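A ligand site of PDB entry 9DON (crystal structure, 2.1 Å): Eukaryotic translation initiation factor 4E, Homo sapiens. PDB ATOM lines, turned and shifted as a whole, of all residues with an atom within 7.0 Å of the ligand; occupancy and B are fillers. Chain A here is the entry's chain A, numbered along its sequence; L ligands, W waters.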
ATOM      1  N   PHE A  22       1.863 -11.580 -13.540  1.00  0.00           N
ATOM      2  CA  PHE A  22       1.566 -10.354 -12.866  1.00  0.00           C
ATOM      3  C   PHE A  22       0.070 -10.313 -12.669  1.00  0.00           C
ATOM      4  O   PHE A  22      -0.683 -10.533 -13.609  1.00  0.00           O
ATOM      5  CB  PHE A  22       2.021  -9.146 -13.685  1.00  0.00           C
ATOM      6  CG  PHE A  22       1.719  -7.824 -13.023  1.00  0.00           C
ATOM      7  CD1 PHE A  22       0.494  -7.216 -13.181  1.00  0.00           C
ATOM      8  CD2 PHE A  22       2.680  -7.177 -12.270  1.00  0.00           C
ATOM      9  CE1 PHE A  22       0.210  -6.020 -12.532  1.00  0.00           C
ATOM     10  CE2 PHE A  22       2.409  -5.957 -11.678  1.00  0.00           C
ATOM     11  CZ  PHE A  22       1.168  -5.390 -11.780  1.00  0.00           C
ATOM     12  N   ASN A  24      -2.921  -7.752 -10.785  1.00  0.00           N
ATOM     13  CA  ASN A  24      -3.099  -6.459 -10.130  1.00  0.00           C
ATOM     14  C   ASN A  24      -3.701  -6.600  -8.724  1.00  0.00           C
ATOM     15  O   ASN A  24      -4.817  -6.167  -8.492  1.00  0.00           O
ATOM     16  CB  ASN A  24      -3.868  -5.469 -10.983  1.00  0.00           C
ATOM     17  CG  ASN A  24      -3.249  -4.105 -10.855  1.00  0.00           C
ATOM     18  OD1 ASN A  24      -3.007  -3.592  -9.742  1.00  0.00           O
ATOM     19  ND2 ASN A  24      -2.925  -3.515 -12.005  1.00  0.00           N
ATOM     20  N   TRP A  30       3.634  -2.618  -7.505  1.00  0.00           N
ATOM     21  CA  TRP A  30       3.910  -3.217  -8.815  1.00  0.00           C
ATOM     22  C   TRP A  30       4.925  -4.355  -8.762  1.00  0.00           C
ATOM     23  O   TRP A  30       4.627  -5.446  -9.227  1.00  0.00           O
ATOM     24  CB  TRP A  30       4.335  -2.147  -9.853  1.00  0.00           C
ATOM     25  CG  TRP A  30       4.309  -2.676 -11.258  1.00  0.00           C
ATOM     26  CD1 TRP A  30       3.253  -2.661 -12.119  1.00  0.00           C
ATOM     27  CD2 TRP A  30       5.363  -3.398 -11.936  1.00  0.00           C
ATOM     28  NE1 TRP A  30       3.550  -3.387 -13.249  1.00  0.00           N
ATOM     29  CE2 TRP A  30       4.850  -3.797 -13.185  1.00  0.00           C
ATOM     30  CE3 TRP A  30       6.680  -3.728 -11.612  1.00  0.00           C
ATOM     31  CZ2 TRP A  30       5.606  -4.536 -14.092  1.00  0.00           C
ATOM     32  CZ3 TRP A  30       7.433  -4.443 -12.513  1.00  0.00           C
ATOM     33  CH2 TRP A  30       6.901  -4.852 -13.732  1.00  0.00           C
ATOM     34  N   GLN A  31       6.107  -4.106  -8.161  1.00  0.00           N
ATOM     35  CA  GLN A  31       7.144  -5.125  -8.100  1.00  0.00           C
ATOM     36  C   GLN A  31       6.775  -6.345  -7.274  1.00  0.00           C
ATOM     37  O   GLN A  31       7.128  -7.447  -7.663  1.00  0.00           O
ATOM     38  CB  GLN A  31       8.478  -4.520  -7.616  1.00  0.00           C
ATOM     39  CG  GLN A  31       9.284  -3.848  -8.735  1.00  0.00           C
ATOM     40  CD  GLN A  31      10.669  -3.483  -8.240  1.00  0.00           C
ATOM     41  OE1 GLN A  31      11.366  -4.302  -7.636  1.00  0.00           O
ATOM     42  NE2 GLN A  31      11.086  -2.270  -8.474  1.00  0.00           N
ATOM     43  N   LEU A  34       4.704  -8.915  -9.354  1.00  0.00           N
ATOM     44  CA  LEU A  34       5.373  -9.595 -10.461  1.00  0.00           C
ATOM     45  C   LEU A  34       6.051 -10.843  -9.913  1.00  0.00           C
ATOM     46  O   LEU A  34       7.088 -10.711  -9.256  1.00  0.00           O
ATOM     47  CB  LEU A  34       6.438  -8.659 -11.034  1.00  0.00           C
ATOM     48  CG  LEU A  34       7.242  -9.196 -12.201  1.00  0.00           C
ATOM     49  CD1 LEU A  34       6.335  -9.501 -13.384  1.00  0.00           C
ATOM     50  CD2 LEU A  34       8.383  -8.225 -12.548  1.00  0.00           C
ATOM     51  N   GLY A  62      -5.953  -6.654 -16.611  1.00  0.00           N
ATOM     52  CA  GLY A  62      -4.918  -6.185 -15.691  1.00  0.00           C
ATOM     53  C   GLY A  62      -3.832  -7.211 -15.401  1.00  0.00           C
ATOM     54  O   GLY A  62      -2.855  -6.898 -14.728  1.00  0.00           O
ATOM     55  N   ASP A  64      -0.767 -10.108 -16.576  1.00  0.00           N
ATOM     56  CA  ASP A  64       0.268 -10.294 -17.565  1.00  0.00           C
ATOM     57  C   ASP A  64       0.935 -11.640 -17.382  1.00  0.00           C
ATOM     58  O   ASP A  64       1.120 -12.077 -16.260  1.00  0.00           O
ATOM     59  CB  ASP A  64       1.415  -9.281 -17.386  1.00  0.00           C
ATOM     60  CG  ASP A  64       1.143  -7.795 -17.261  1.00  0.00           C
ATOM     61  OD1 ASP A  64       0.159  -7.322 -17.859  1.00  0.00           O
ATOM     62  OD2 ASP A  64       1.999  -7.078 -16.647  1.00  0.00           O
ATOM     63  N   PRO A  74      11.429  -9.659 -15.447  1.00  0.00           N
ATOM     64  CA  PRO A  74      10.691  -8.905 -16.468  1.00  0.00           C
ATOM     65  C   PRO A  74      10.333  -7.473 -16.079  1.00  0.00           C
ATOM     66  O   PRO A  74       9.161  -7.087 -16.055  1.00  0.00           O
ATOM     67  CB  PRO A  74       9.441  -9.737 -16.695  1.00  0.00           C
ATOM     68  CG  PRO A  74       9.234 -10.467 -15.437  1.00  0.00           C
ATOM     69  CD  PRO A  74      10.559 -10.633 -14.758  1.00  0.00           C
ATOM     70  N   MET A  75      11.345  -6.677 -15.784  1.00  0.00           N
ATOM     71  CA  MET A  75      11.172  -5.290 -15.414  1.00  0.00           C
ATOM     72  C   MET A  75      12.328  -4.446 -15.930  1.00  0.00           C
ATOM     73  O   MET A  75      13.439  -4.961 -16.139  1.00  0.00           O
ATOM     74  CB  MET A  75      10.954  -5.140 -13.900  1.00  0.00           C
ATOM     75  CG  MET A  75      12.098  -5.605 -13.070  1.00  0.00           C
ATOM     76  SD  MET A  75      11.756  -5.450 -11.271  1.00  0.00           S
ATOM     77  CE  MET A  75      13.267  -6.154 -10.640  1.00  0.00           C
ATOM     78  N   TRP A  76      12.053  -3.165 -16.180  1.00  0.00           N
ATOM     79  CA  TRP A  76      13.029  -2.192 -16.699  1.00  0.00           C
ATOM     80  C   TRP A  76      14.258  -2.089 -15.789  1.00  0.00           C
ATOM     81  O   TRP A  76      15.353  -1.830 -16.282  1.00  0.00           O
ATOM     82  CB  TRP A  76      12.411  -0.783 -16.816  1.00  0.00           C
ATOM     83  CG  TRP A  76      11.070  -0.668 -17.486  1.00  0.00           C
ATOM     84  CD1 TRP A  76      10.663  -1.277 -18.631  1.00  0.00           C
ATOM     85  CD2 TRP A  76      10.030   0.260 -17.130  1.00  0.00           C
ATOM     86  NE1 TRP A  76       9.421  -0.817 -19.002  1.00  0.00           N
ATOM     87  CE2 TRP A  76       9.007   0.122 -18.089  1.00  0.00           C
ATOM     88  CE3 TRP A  76       9.832   1.136 -16.068  1.00  0.00           C
ATOM     89  CZ2 TRP A  76       7.808   0.839 -18.014  1.00  0.00           C
ATOM     90  CZ3 TRP A  76       8.656   1.862 -15.999  1.00  0.00           C
ATOM     91  CH2 TRP A  76       7.666   1.718 -16.974  1.00  0.00           C
ATOM     92  N   GLU A  77      14.066  -2.261 -14.474  1.00  0.00           N
ATOM     93  CA  GLU A  77      15.079  -2.162 -13.418  1.00  0.00           C
ATOM     94  C   GLU A  77      16.178  -3.199 -13.538  1.00  0.00           C
ATOM     95  O   GLU A  77      17.297  -2.952 -13.095  1.00  0.00           O
ATOM     96  CB  GLU A  77      14.427  -2.287 -12.026  1.00  0.00           C
ATOM     97  CG  GLU A  77      13.521  -1.115 -11.647  1.00  0.00           C
ATOM     98  CD  GLU A  77      12.068  -1.204 -12.099  1.00  0.00           C
ATOM     99  OE1 GLU A  77      11.788  -1.875 -13.111  1.00  0.00           O
ATOM    100  OE2 GLU A  77      11.212  -0.577 -11.442  1.00  0.00           O
ATOM    101  N   ASP A  78      15.879  -4.364 -14.141  1.00  0.00           N
ATOM    102  CA  ASP A  78      16.898  -5.418 -14.303  1.00  0.00           C
ATOM    103  C   ASP A  78      18.031  -4.894 -15.185  1.00  0.00           C
ATOM    104  O   ASP A  78      17.774  -4.194 -16.158  1.00  0.00           O
ATOM    105  CB  ASP A  78      16.281  -6.666 -14.957  1.00  0.00           C
ATOM    106  CG  ASP A  78      17.154  -7.884 -14.818  1.00  0.00           C
ATOM    107  OD1 ASP A  78      18.189  -7.976 -15.523  1.00  0.00           O
ATOM    108  OD2 ASP A  78      16.814  -8.778 -14.009  1.00  0.00           O
ATOM    109  N   ARG A  86      11.512  -2.513 -26.260  1.00  0.00           N
ATOM    110  CA  ARG A  86      10.588  -3.558 -26.704  1.00  0.00           C
ATOM    111  C   ARG A  86       9.931  -3.265 -28.036  1.00  0.00           C
ATOM    112  O   ARG A  86       9.624  -2.113 -28.368  1.00  0.00           O
ATOM    113  CB  ARG A  86       9.479  -3.751 -25.640  1.00  0.00           C
ATOM    114  CG  ARG A  86       8.669  -2.448 -25.384  1.00  0.00           C
ATOM    115  CD  ARG A  86       7.489  -2.638 -24.436  1.00  0.00           C
ATOM    116  NE  ARG A  86       6.841  -1.361 -24.170  1.00  0.00           N
ATOM    117  CZ  ARG A  86       5.651  -1.214 -23.580  1.00  0.00           C
ATOM    118  NH1 ARG A  86       4.978  -2.278 -23.167  1.00  0.00           N
ATOM    119  NH2 ARG A  86       5.141  -0.004 -23.392  1.00  0.00           N
ATOM    120  N   VAL A 127       6.351 -10.312 -23.171  1.00  0.00           N
ATOM    121  CA  VAL A 127       5.294 -10.038 -22.201  1.00  0.00           C
ATOM    122  C   VAL A 127       3.965  -9.932 -22.943  1.00  0.00           C
ATOM    123  O   VAL A 127       3.890  -9.291 -23.997  1.00  0.00           O
ATOM    124  CB  VAL A 127       5.556  -8.679 -21.480  1.00  0.00           C
ATOM    125  CG1 VAL A 127       4.456  -8.353 -20.468  1.00  0.00           C
ATOM    126  CG2 VAL A 127       6.940  -8.632 -20.818  1.00  0.00           C
ATOM    127  N   ASN A 129       0.146  -8.441 -22.117  1.00  0.00           N
ATOM    128  CA  ASN A 129      -0.714  -7.670 -21.224  1.00  0.00           C
ATOM    129  C   ASN A 129      -2.154  -7.892 -21.669  1.00  0.00           C
ATOM    130  O   ASN A 129      -2.512  -7.598 -22.810  1.00  0.00           O
ATOM    131  CB  ASN A 129      -0.399  -6.186 -21.330  1.00  0.00           C
ATOM    132  CG  ASN A 129       1.046  -5.859 -21.071  1.00  0.00           C
ATOM    133  OD1 ASN A 129       1.785  -5.424 -21.960  1.00  0.00           O
ATOM    134  ND2 ASN A 129       1.491  -6.074 -19.863  1.00  0.00           N
ATOM    135  N   ARG A 131      -5.785  -6.620 -21.289  1.00  0.00           N
ATOM    136  CA  ARG A 131      -6.442  -5.367 -20.888  1.00  0.00           C
ATOM    137  C   ARG A 131      -7.773  -5.210 -21.600  1.00  0.00           C
ATOM    138  O   ARG A 131      -7.897  -5.588 -22.781  1.00  0.00           O
ATOM    139  CB  ARG A 131      -5.572  -4.154 -21.264  1.00  0.00           C
ATOM    140  CG  ARG A 131      -4.149  -4.121 -20.677  1.00  0.00           C
ATOM    141  CD  ARG A 131      -4.156  -3.868 -19.189  1.00  0.00           C
ATOM    142  NE  ARG A 131      -2.807  -3.706 -18.628  1.00  0.00           N
ATOM    143  CZ  ARG A 131      -2.044  -4.720 -18.209  1.00  0.00           C
ATOM    144  NH1 ARG A 131      -2.474  -5.974 -18.319  1.00  0.00           N
ATOM    145  NH2 ARG A 131      -0.834  -4.487 -17.710  1.00  0.00           N
ATOM    146  N   GLY A 134      -7.534  -3.070 -24.728  1.00  0.00           N
ATOM    147  CA  GLY A 134      -6.824  -3.681 -25.843  1.00  0.00           C
ATOM    148  C   GLY A 134      -5.602  -4.432 -25.375  1.00  0.00           C
ATOM    149  O   GLY A 134      -4.792  -3.911 -24.600  1.00  0.00           O
ATOM    150  N   LYS A 136      -1.852  -6.366 -25.506  1.00  0.00           N
ATOM    151  CA  LYS A 136      -0.529  -6.023 -26.040  1.00  0.00           C
ATOM    152  C   LYS A 136       0.443  -7.190 -25.882  1.00  0.00           C
ATOM    153  O   LYS A 136       0.417  -7.880 -24.870  1.00  0.00           O
ATOM    154  CB  LYS A 136       0.051  -4.785 -25.317  1.00  0.00           C
ATOM    155  CG  LYS A 136      -0.765  -3.499 -25.502  1.00  0.00           C
ATOM    156  CD  LYS A 136      -0.100  -2.327 -24.818  1.00  0.00           C
ATOM    157  CE  LYS A 136      -0.749  -1.981 -23.518  1.00  0.00           C
ATOM    158  NZ  LYS A 136       0.112  -1.103 -22.682  1.00  0.00           N
ATOM    159  N   TRP A 140      11.113  -8.046 -25.584  1.00  0.00           N
ATOM    160  CA  TRP A 140      12.074  -7.201 -24.889  1.00  0.00           C
ATOM    161  C   TRP A 140      13.500  -7.535 -25.288  1.00  0.00           C
ATOM    162  O   TRP A 140      13.884  -8.714 -25.300  1.00  0.00           O
ATOM    163  CB  TRP A 140      11.903  -7.383 -23.387  1.00  0.00           C
ATOM    164  CG  TRP A 140      10.731  -6.657 -22.799  1.00  0.00           C
ATOM    165  CD1 TRP A 140       9.502  -6.488 -23.344  1.00  0.00           C
ATOM    166  CD2 TRP A 140      10.677  -6.058 -21.507  1.00  0.00           C
ATOM    167  NE1 TRP A 140       8.666  -5.856 -22.462  1.00  0.00           N
ATOM    168  CE2 TRP A 140       9.376  -5.563 -21.333  1.00  0.00           C
ATOM    169  CE3 TRP A 140      11.602  -5.919 -20.460  1.00  0.00           C
ATOM    170  CZ2 TRP A 140       8.986  -4.905 -20.158  1.00  0.00           C
ATOM    171  CZ3 TRP A 140      11.203  -5.299 -19.303  1.00  0.00           C
ATOM    172  CH2 TRP A 140       9.909  -4.792 -19.157  1.00  0.00           C
ATOM    173  N   HIS A 174      13.054   1.443 -23.032  1.00  0.00           N
ATOM    174  CA  HIS A 174      12.461   1.400 -21.700  1.00  0.00           C
ATOM    175  C   HIS A 174      12.675   2.725 -20.968  1.00  0.00           C
ATOM    176  O   HIS A 174      11.819   3.114 -20.183  1.00  0.00           O
ATOM    177  CB  HIS A 174      13.039   0.240 -20.849  1.00  0.00           C
ATOM    178  CG  HIS A 174      12.671  -1.116 -21.378  1.00  0.00           C
ATOM    179  ND1 HIS A 174      11.422  -1.371 -21.870  1.00  0.00           N
ATOM    180  CD2 HIS A 174      13.418  -2.235 -21.472  1.00  0.00           C
ATOM    181  CE1 HIS A 174      11.434  -2.652 -22.235  1.00  0.00           C
ATOM    182  NE2 HIS A 174      12.625  -3.203 -22.031  1.00  0.00           N
ATOM    183  N   THR A 177       9.825   4.862 -22.146  1.00  0.00           N
ATOM    184  CA  THR A 177       8.544   4.444 -21.569  1.00  0.00           C
ATOM    185  C   THR A 177       8.450   4.867 -20.099  1.00  0.00           C
ATOM    186  O   THR A 177       7.410   5.391 -19.674  1.00  0.00           O
ATOM    187  CB  THR A 177       8.365   2.916 -21.650  1.00  0.00           C
ATOM    188  OG1 THR A 177       8.629   2.498 -22.970  1.00  0.00           O
ATOM    189  CG2 THR A 177       6.976   2.481 -21.220  1.00  0.00           C
HETATM  190  P1  LIG L   1       1.837  -1.436 -18.479  1.00  0.00           P
HETATM  191  O1  LIG L   1       1.172  -2.387 -17.570  1.00  0.00           O
HETATM  192  O2  LIG L   1       2.993  -2.008 -19.315  1.00  0.00           O
HETATM  193  O3  LIG L   1       0.782  -0.806 -19.481  1.00  0.00           O
HETATM  194  O4  LIG L   1       2.398  -0.164 -17.664  1.00  0.00           O
HETATM  195  P2  LIG L   1      -0.782  -0.426 -19.396  1.00  0.00           P
HETATM  196  O5  LIG L   1      -1.562  -1.158 -20.447  1.00  0.00           O
HETATM  197  O6  LIG L   1      -0.803   1.101 -19.541  1.00  0.00           O
HETATM  198  O7  LIG L   1      -1.190  -0.781 -17.979  1.00  0.00           O
HETATM  199  C1  LIG L   1       1.554   0.668 -16.851  1.00  0.00           C
HETATM  200  C2  LIG L   1       2.315   1.038 -15.593  1.00  0.00           C
HETATM  201  O8  LIG L   1       2.884  -0.162 -15.008  1.00  0.00           O
HETATM  202  C3  LIG L   1       3.518   1.948 -15.820  1.00  0.00           C
HETATM  203  O9  LIG L   1       3.126   3.313 -15.915  1.00  0.00           O
HETATM  204  C4  LIG L   1       4.364   1.650 -14.591  1.00  0.00           C
HETATM  205  O10 LIG L   1       3.883   2.338 -13.432  1.00  0.00           O
HETATM  206  C5  LIG L   1       4.139   0.139 -14.414  1.00  0.00           C
HETATM  207  N1  LIG L   1       5.247  -0.601 -14.976  1.00  0.00           N
HETATM  208  C6  LIG L   1       5.018  -1.549 -16.045  1.00  0.00           C
HETATM  209  N2  LIG L   1       6.360  -1.967 -16.348  1.00  0.00           N
HETATM  210  C7  LIG L   1       6.550  -3.010 -17.342  1.00  0.00           C
HETATM  211  C8  LIG L   1       7.196  -1.645 -15.297  1.00  0.00           C
HETATM  212  C9  LIG L   1       8.535  -2.008 -14.985  1.00  0.00           C
HETATM  213  O11 LIG L   1       9.297  -2.730 -15.620  1.00  0.00           O
HETATM  214  N3  LIG L   1       8.930  -1.471 -13.783  1.00  0.00           N
HETATM  215  C10 LIG L   1       8.139  -0.728 -12.937  1.00  0.00           C
HETATM  216  N4  LIG L   1       8.679  -0.351 -11.784  1.00  0.00           N
HETATM  217  N5  LIG L   1       6.879  -0.395 -13.206  1.00  0.00           N
HETATM  218  C11 LIG L   1       6.456  -0.862 -14.391  1.00  0.00           C
HETATM  219  O   HOH W   1       2.276  -2.425 -21.879  1.00  0.00           O
HETATM  220  O   HOH W   2       4.969  -0.249 -19.807  1.00  0.00           O
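Water W1 lies within hydrogen-bond range of the side-chain amino group of Lys 136, an oxygen (O2) of the ligand, the guanidinium group of Arg 86 and the side-chain amide oxygen of Asn 129.
The guanidinium group (NH2) of Arg 131 is in salt-bridge range of an oxygen (O1) of the ligand (2.9 Å). A nitrogen (N4) of the ligand sits at hydrogen-bond distance from the side-chain carboxylate (OE2) of Glu 77 (2.6 Å). The side-chain amino group (NZ) of Lys 136 lies within salt-bridge range of an oxygen (O5) of the ligand (2.8 Å). The backbone NH (N) of Trp 76 sits at hydrogen-bond distance from an oxygen (O11) of the ligand (2.8 Å).
Trp 30 touches the ligand (CZ2 to N2, 3.5 Å). CA of Met 75 touches O11 of the ligand, at 3.2 Å. Of the 21 residues printed, 6 come within 4 Å of the ligand. The nearest printed residue that does not touch the ligand is Trp 140 (4.1 Å).
The backbone carbonyl oxygen (O) of Lys 136 is in hydrogen-bond range of the backbone NH (N) of Asn 129 (2.8 Å). The guanidinium group (NH1) of Arg 131 lies within salt-bridge range of the side-chain carboxylate (OD1) of Asp 64 (3.0 Å). The side-chain amide nitrogen (NE2) of Gln 31 lies within hydrogen-bond range of the side-chain carboxylate (OE2) of Glu 77 (3.4 Å).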
